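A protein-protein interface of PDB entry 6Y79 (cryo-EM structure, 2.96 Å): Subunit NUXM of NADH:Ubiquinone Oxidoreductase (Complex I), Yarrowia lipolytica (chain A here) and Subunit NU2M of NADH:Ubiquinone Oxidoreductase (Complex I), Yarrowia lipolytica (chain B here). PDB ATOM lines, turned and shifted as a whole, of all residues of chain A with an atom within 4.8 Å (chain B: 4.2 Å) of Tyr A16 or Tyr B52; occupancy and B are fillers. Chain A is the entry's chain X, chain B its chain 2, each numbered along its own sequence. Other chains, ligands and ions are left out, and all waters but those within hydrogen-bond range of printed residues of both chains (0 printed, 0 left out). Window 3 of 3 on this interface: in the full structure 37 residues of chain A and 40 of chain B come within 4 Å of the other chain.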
ATOM      1  N   TYR A  14     -28.253  22.320   3.641  1.00  0.00           N
ATOM      2  CA  TYR A  14     -27.342  23.025   4.532  1.00  0.00           C
ATOM      3  C   TYR A  14     -25.931  22.557   4.222  1.00  0.00           C
ATOM      4  O   TYR A  14     -25.421  21.618   4.826  1.00  0.00           O
ATOM      5  CB  TYR A  14     -27.727  22.755   5.980  1.00  0.00           C
ATOM      6  CG  TYR A  14     -26.899  23.464   7.014  1.00  0.00           C
ATOM      7  CD1 TYR A  14     -27.204  24.751   7.414  1.00  0.00           C
ATOM      8  CD2 TYR A  14     -25.820  22.838   7.606  1.00  0.00           C
ATOM      9  CE1 TYR A  14     -26.440  25.388   8.362  1.00  0.00           C
ATOM     10  CE2 TYR A  14     -25.054  23.464   8.519  1.00  0.00           C
ATOM     11  CZ  TYR A  14     -25.367  24.720   8.911  1.00  0.00           C
ATOM     12  OH  TYR A  14     -24.569  25.287   9.859  1.00  0.00           O
ATOM     13  N   SER A  15     -25.280  23.215   3.271  1.00  0.00           N
ATOM     14  CA  SER A  15     -23.986  22.725   2.820  1.00  0.00           C
ATOM     15  C   SER A  15     -22.888  23.088   3.809  1.00  0.00           C
ATOM     16  O   SER A  15     -22.878  24.178   4.388  1.00  0.00           O
ATOM     17  CB  SER A  15     -23.644  23.281   1.441  1.00  0.00           C
ATOM     18  OG  SER A  15     -22.347  22.866   1.073  1.00  0.00           O
ATOM     19  N   TYR A  16     -21.953  22.163   3.977  1.00  0.00           N
ATOM     20  CA  TYR A  16     -20.883  22.236   4.958  1.00  0.00           C
ATOM     21  C   TYR A  16     -19.616  22.868   4.414  1.00  0.00           C
ATOM     22  O   TYR A  16     -18.631  22.981   5.149  1.00  0.00           O
ATOM     23  CB  TYR A  16     -20.554  20.836   5.465  1.00  0.00           C
ATOM     24  CG  TYR A  16     -21.702  20.155   6.139  1.00  0.00           C
ATOM     25  CD1 TYR A  16     -21.951  20.364   7.475  1.00  0.00           C
ATOM     26  CD2 TYR A  16     -22.543  19.310   5.437  1.00  0.00           C
ATOM     27  CE1 TYR A  16     -22.991  19.748   8.094  1.00  0.00           C
ATOM     28  CE2 TYR A  16     -23.599  18.691   6.056  1.00  0.00           C
ATOM     29  CZ  TYR A  16     -23.814  18.915   7.386  1.00  0.00           C
ATOM     30  OH  TYR A  16     -24.864  18.304   8.020  1.00  0.00           O
ATOM     31  N   GLY A  17     -19.607  23.252   3.157  1.00  0.00           N
ATOM     32  CA  GLY A  17     -18.443  23.855   2.536  1.00  0.00           C
ATOM     33  C   GLY A  17     -18.892  24.777   1.445  1.00  0.00           C
ATOM     34  O   GLY A  17     -19.979  25.359   1.515  1.00  0.00           O
ATOM     35  N   ASP A  18     -18.049  24.923   0.426  1.00  0.00           N
ATOM     36  CA  ASP A  18     -18.425  25.732  -0.724  1.00  0.00           C
ATOM     37  C   ASP A  18     -19.476  25.034  -1.571  1.00  0.00           C
ATOM     38  O   ASP A  18     -20.418  25.672  -2.054  1.00  0.00           O
ATOM     39  CB  ASP A  18     -17.188  26.044  -1.555  1.00  0.00           C
ATOM     40  CG  ASP A  18     -16.288  24.835  -1.730  1.00  0.00           C
ATOM     41  OD1 ASP A  18     -16.655  23.736  -1.263  1.00  0.00           O
ATOM     42  OD2 ASP A  18     -15.211  24.991  -2.344  1.00  0.00           O
ATOM     43  N   LEU A  21     -24.383  19.953  -0.871  1.00  0.00           N
ATOM     44  CA  LEU A  21     -24.355  18.626  -0.286  1.00  0.00           C
ATOM     45  C   LEU A  21     -25.112  17.639  -1.157  1.00  0.00           C
ATOM     46  O   LEU A  21     -25.977  17.999  -1.957  1.00  0.00           O
ATOM     47  CB  LEU A  21     -24.929  18.616   1.136  1.00  0.00           C
ATOM     48  CG  LEU A  21     -26.400  18.716   1.547  1.00  0.00           C
ATOM     49  CD1 LEU A  21     -27.112  17.397   1.608  1.00  0.00           C
ATOM     50  CD2 LEU A  21     -26.435  19.261   2.915  1.00  0.00           C
ATOM     51  N   ALA A  24     -26.685  13.870   3.948  1.00  0.00           N
ATOM     52  CA  ALA A  24     -26.240  14.214   5.288  1.00  0.00           C
ATOM     53  C   ALA A  24     -25.659  13.023   6.030  1.00  0.00           C
ATOM     54  O   ALA A  24     -24.853  13.211   6.947  1.00  0.00           O
ATOM     55  CB  ALA A  24     -27.383  14.817   6.088  1.00  0.00           C
ATOM     56  N   PHE A  99     -20.849  15.398   1.662  1.00  0.00           N
ATOM     57  CA  PHE A  99     -21.166  16.543   2.508  1.00  0.00           C
ATOM     58  C   PHE A  99     -20.962  17.874   1.806  1.00  0.00           C
ATOM     59  O   PHE A  99     -21.483  18.890   2.273  1.00  0.00           O
ATOM     60  CB  PHE A  99     -20.332  16.523   3.783  1.00  0.00           C
ATOM     61  CG  PHE A  99     -20.664  15.397   4.701  1.00  0.00           C
ATOM     62  CD1 PHE A  99     -21.854  14.705   4.583  1.00  0.00           C
ATOM     63  CD2 PHE A  99     -19.784  15.026   5.684  1.00  0.00           C
ATOM     64  CE1 PHE A  99     -22.140  13.668   5.409  1.00  0.00           C
ATOM     65  CE2 PHE A  99     -20.083  13.996   6.520  1.00  0.00           C
ATOM     66  CZ  PHE A  99     -21.257  13.315   6.383  1.00  0.00           C
ATOM     67  N   GLY A 100     -20.232  17.896   0.702  1.00  0.00           N
ATOM     68  CA  GLY A 100     -19.992  19.137   0.013  1.00  0.00           C
ATOM     69  C   GLY A 100     -18.863  19.953   0.578  1.00  0.00           C
ATOM     70  O   GLY A 100     -18.888  21.180   0.470  1.00  0.00           O
ATOM     71  N   VAL A 101     -17.875  19.316   1.195  1.00  0.00           N
ATOM     72  CA  VAL A 101     -16.699  20.036   1.655  1.00  0.00           C
ATOM     73  C   VAL A 101     -15.539  19.910   0.677  1.00  0.00           C
ATOM     74  O   VAL A 101     -14.586  20.696   0.767  1.00  0.00           O
ATOM     75  CB  VAL A 101     -16.268  19.575   3.063  1.00  0.00           C
ATOM     76  CG1 VAL A 101     -17.416  19.649   4.027  1.00  0.00           C
ATOM     77  CG2 VAL A 101     -15.749  18.197   3.022  1.00  0.00           C
ATOM     78  N   HIS A 145     -23.340  12.033  10.867  1.00  0.00           N
ATOM     79  CA  HIS A 145     -22.041  12.705  10.951  1.00  0.00           C
ATOM     80  C   HIS A 145     -21.019  11.891  11.726  1.00  0.00           C
ATOM     81  O   HIS A 145     -20.166  12.446  12.413  1.00  0.00           O
ATOM     82  CB  HIS A 145     -22.174  14.104  11.551  1.00  0.00           C
ATOM     83  CG  HIS A 145     -23.181  14.955  10.856  1.00  0.00           C
ATOM     84  ND1 HIS A 145     -24.396  15.276  11.415  1.00  0.00           N
ATOM     85  CD2 HIS A 145     -23.166  15.524   9.629  1.00  0.00           C
ATOM     86  CE1 HIS A 145     -25.077  16.025  10.571  1.00  0.00           C
ATOM     87  NE2 HIS A 145     -24.355  16.189   9.478  1.00  0.00           N
ATOM     88  N   ALA A 148     -16.800  12.208  11.294  1.00  0.00           N
ATOM     89  CA  ALA A 148     -16.014  12.825  12.341  1.00  0.00           C
ATOM     90  C   ALA A 148     -15.916  11.821  13.469  1.00  0.00           C
ATOM     91  O   ALA A 148     -16.854  11.065  13.716  1.00  0.00           O
ATOM     92  CB  ALA A 148     -16.669  14.121  12.806  1.00  0.00           C
ATOM     93  N   LEU B  45     -13.789  19.194   7.806  1.00  0.00           N
ATOM     94  CA  LEU B  45     -15.158  19.166   8.307  1.00  0.00           C
ATOM     95  C   LEU B  45     -15.459  20.367   9.181  1.00  0.00           C
ATOM     96  O   LEU B  45     -16.592  20.853   9.200  1.00  0.00           O
ATOM     97  CB  LEU B  45     -15.403  17.894   9.110  1.00  0.00           C
ATOM     98  CG  LEU B  45     -15.614  16.570   8.397  1.00  0.00           C
ATOM     99  CD1 LEU B  45     -15.700  15.482   9.434  1.00  0.00           C
ATOM    100  CD2 LEU B  45     -16.871  16.606   7.559  1.00  0.00           C
ATOM    101  N   PHE B  46     -14.469  20.847   9.914  1.00  0.00           N
ATOM    102  CA  PHE B  46     -14.672  21.849  10.952  1.00  0.00           C
ATOM    103  C   PHE B  46     -14.278  23.242  10.471  1.00  0.00           C
ATOM    104  O   PHE B  46     -13.406  23.890  11.023  1.00  0.00           O
ATOM    105  CB  PHE B  46     -13.892  21.451  12.192  1.00  0.00           C
ATOM    106  CG  PHE B  46     -14.217  20.082  12.682  1.00  0.00           C
ATOM    107  CD1 PHE B  46     -15.437  19.829  13.267  1.00  0.00           C
ATOM    108  CD2 PHE B  46     -13.321  19.043  12.539  1.00  0.00           C
ATOM    109  CE1 PHE B  46     -15.755  18.581  13.704  1.00  0.00           C
ATOM    110  CE2 PHE B  46     -13.643  17.788  12.980  1.00  0.00           C
ATOM    111  CZ  PHE B  46     -14.856  17.560  13.560  1.00  0.00           C
ATOM    112  N   LEU B  47     -14.956  23.715   9.437  1.00  0.00           N
ATOM    113  CA  LEU B  47     -14.811  25.092   8.996  1.00  0.00           C
ATOM    114  C   LEU B  47     -15.725  25.984   9.815  1.00  0.00           C
ATOM    115  O   LEU B  47     -16.870  25.617  10.088  1.00  0.00           O
ATOM    116  CB  LEU B  47     -15.171  25.238   7.521  1.00  0.00           C
ATOM    117  CG  LEU B  47     -14.243  24.800   6.395  1.00  0.00           C
ATOM    118  CD1 LEU B  47     -14.993  24.869   5.077  1.00  0.00           C
ATOM    119  CD2 LEU B  47     -13.070  25.705   6.334  1.00  0.00           C
ATOM    120  N   GLN B  50     -17.787  24.801  12.942  1.00  0.00           N
ATOM    121  CA  GLN B  50     -18.922  23.910  12.779  1.00  0.00           C
ATOM    122  C   GLN B  50     -18.749  22.729  13.721  1.00  0.00           C
ATOM    123  O   GLN B  50     -17.716  22.057  13.700  1.00  0.00           O
ATOM    124  CB  GLN B  50     -19.045  23.440  11.335  1.00  0.00           C
ATOM    125  CG  GLN B  50     -20.191  22.475  11.109  1.00  0.00           C
ATOM    126  CD  GLN B  50     -21.533  23.096  11.387  1.00  0.00           C
ATOM    127  OE1 GLN B  50     -22.179  22.783  12.380  1.00  0.00           O
ATOM    128  NE2 GLN B  50     -21.961  23.986  10.510  1.00  0.00           N
ATOM    129  N   THR B  51     -19.752  22.484  14.546  1.00  0.00           N
ATOM    130  CA  THR B  51     -19.702  21.461  15.570  1.00  0.00           C
ATOM    131  C   THR B  51     -20.760  20.401  15.296  1.00  0.00           C
ATOM    132  O   THR B  51     -21.893  20.718  14.931  1.00  0.00           O
ATOM    133  CB  THR B  51     -19.916  22.098  16.938  1.00  0.00           C
ATOM    134  OG1 THR B  51     -18.943  23.128  17.145  1.00  0.00           O
ATOM    135  CG2 THR B  51     -19.799  21.107  18.031  1.00  0.00           C
ATOM    136  N   TYR B  52     -20.377  19.137  15.450  1.00  0.00           N
ATOM    137  CA  TYR B  52     -21.264  18.004  15.259  1.00  0.00           C
ATOM    138  C   TYR B  52     -21.540  17.343  16.597  1.00  0.00           C
ATOM    139  O   TYR B  52     -20.704  17.368  17.495  1.00  0.00           O
ATOM    140  CB  TYR B  52     -20.643  16.982  14.315  1.00  0.00           C
ATOM    141  CG  TYR B  52     -20.346  17.520  12.947  1.00  0.00           C
ATOM    142  CD1 TYR B  52     -21.179  18.439  12.351  1.00  0.00           C
ATOM    143  CD2 TYR B  52     -19.223  17.121  12.255  1.00  0.00           C
ATOM    144  CE1 TYR B  52     -20.913  18.934  11.102  1.00  0.00           C
ATOM    145  CE2 TYR B  52     -18.947  17.619  11.002  1.00  0.00           C
ATOM    146  CZ  TYR B  52     -19.796  18.527  10.437  1.00  0.00           C
ATOM    147  OH  TYR B  52     -19.534  19.028   9.189  1.00  0.00           O
ATOM    148  N   THR B  53     -22.721  16.755  16.741  1.00  0.00           N
ATOM    149  CA  THR B  53     -22.973  15.833  17.841  1.00  0.00           C
ATOM    150  C   THR B  53     -23.363  14.490  17.257  1.00  0.00           C
ATOM    151  O   THR B  53     -24.193  14.414  16.347  1.00  0.00           O
ATOM    152  CB  THR B  53     -24.038  16.331  18.812  1.00  0.00           C
ATOM    153  OG1 THR B  53     -25.270  16.531  18.123  1.00  0.00           O
ATOM    154  CG2 THR B  53     -23.597  17.609  19.454  1.00  0.00           C
ATOM    155  N   LEU B  59     -21.772  12.246  21.912  1.00  0.00           N
ATOM    156  CA  LEU B  59     -20.431  12.749  21.708  1.00  0.00           C
ATOM    157  C   LEU B  59     -20.514  14.074  20.977  1.00  0.00           C
ATOM    158  O   LEU B  59     -21.436  14.295  20.197  1.00  0.00           O
ATOM    159  CB  LEU B  59     -19.598  11.769  20.906  1.00  0.00           C
ATOM    160  CG  LEU B  59     -19.416  10.396  21.530  1.00  0.00           C
ATOM    161  CD1 LEU B  59     -18.840   9.477  20.508  1.00  0.00           C
ATOM    162  CD2 LEU B  59     -18.510  10.475  22.715  1.00  0.00           C
ATOM    163  N   ILE B  60     -19.561  14.960  21.232  1.00  0.00           N
ATOM    164  CA  ILE B  60     -19.486  16.243  20.547  1.00  0.00           C
ATOM    165  C   ILE B  60     -18.129  16.351  19.862  1.00  0.00           C
ATOM    166  O   ILE B  60     -17.091  16.044  20.456  1.00  0.00           O
ATOM    167  CB  ILE B  60     -19.779  17.417  21.506  1.00  0.00           C
ATOM    168  CG1 ILE B  60     -19.906  18.714  20.737  1.00  0.00           C
ATOM    169  CG2 ILE B  60     -18.779  17.555  22.651  1.00  0.00           C
ATOM    170  CD1 ILE B  60     -20.748  19.733  21.428  1.00  0.00           C
ATOM    171  N   PHE B  61     -18.148  16.694  18.576  1.00  0.00           N
ATOM    172  CA  PHE B  61     -16.950  16.794  17.750  1.00  0.00           C
ATOM    173  C   PHE B  61     -16.877  18.209  17.206  1.00  0.00           C
ATOM    174  O   PHE B  61     -17.663  18.580  16.334  1.00  0.00           O
ATOM    175  CB  PHE B  61     -16.963  15.797  16.589  1.00  0.00           C
ATOM    176  CG  PHE B  61     -16.985  14.353  17.002  1.00  0.00           C
ATOM    177  CD1 PHE B  61     -16.498  13.943  18.204  1.00  0.00           C
ATOM    178  CD2 PHE B  61     -17.483  13.400  16.173  1.00  0.00           C
ATOM    179  CE1 PHE B  61     -16.526  12.619  18.579  1.00  0.00           C
ATOM    180  CE2 PHE B  61     -17.506  12.075  16.561  1.00  0.00           C
ATOM    181  CZ  PHE B  61     -17.017  11.699  17.754  1.00  0.00           C
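OH of Tyr A14 lies within hydrogen-bond range of NE2 of Gln B50, at 3.0 Å.
The side-chain hydroxyl (OH) of Tyr A16 sits at hydrogen-bond distance from a ring nitrogen (NE2) of His A145. The backbone carbonyl oxygen (O) of Leu B45 is in hydrogen-bond range of the side-chain hydroxyl (OH) of Tyr B52 (3.5 Å). O of Tyr B52 is in hydrogen-bond range of N of Phe B61, at 2.9 Å.
Tyr B52 touches Tyr A16 (OH to CD1, 3.3 Å). Leu B45 touches Phe A99. Leu B45 touches Ala A148 (CD1 to CB, 3.8 Å). CB of Ala A148 touches CZ of Phe B46, at 3.96 Å. Ala A148 touches Tyr B52. Ala A148 touches Phe B61.
Of chain B, only Tyr B52 comes within 4 Å of Tyr A16. Tyr B52 touches just these residues of chain A: Tyr A16 and Ala A148. Printed residues of chain A within 4 Å of Gln B50: Tyr A14 (3.0 Å). Of the printed residues of chain B, Ala A148 touches Leu B45, Phe B46, Tyr B52 and Phe B61. Of the printed residues of chain A, Phe B46 touches Ala A148. Gly A17 touches none of the printed residues of chain B. The nearest residue of chain B that does not touch Tyr A16 is Leu B47 (4.1 Å). The nearest printed residue of chain A that does not touch Leu B45 is Val A101 (4.7 Å).
Of the 10 printed residues of chain B, 5 touch a printed residue of chain A. Hydrophobic or aromatic side chains of chain A within 4 Å of the printed part of chain B: Tyr A14, Tyr A16, Phe A99 and Ala A148. Among the printed residues, no Asp or Glu carboxylate lies within 4 Å of a Lys or Arg side-chain nitrogen of the other chain.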
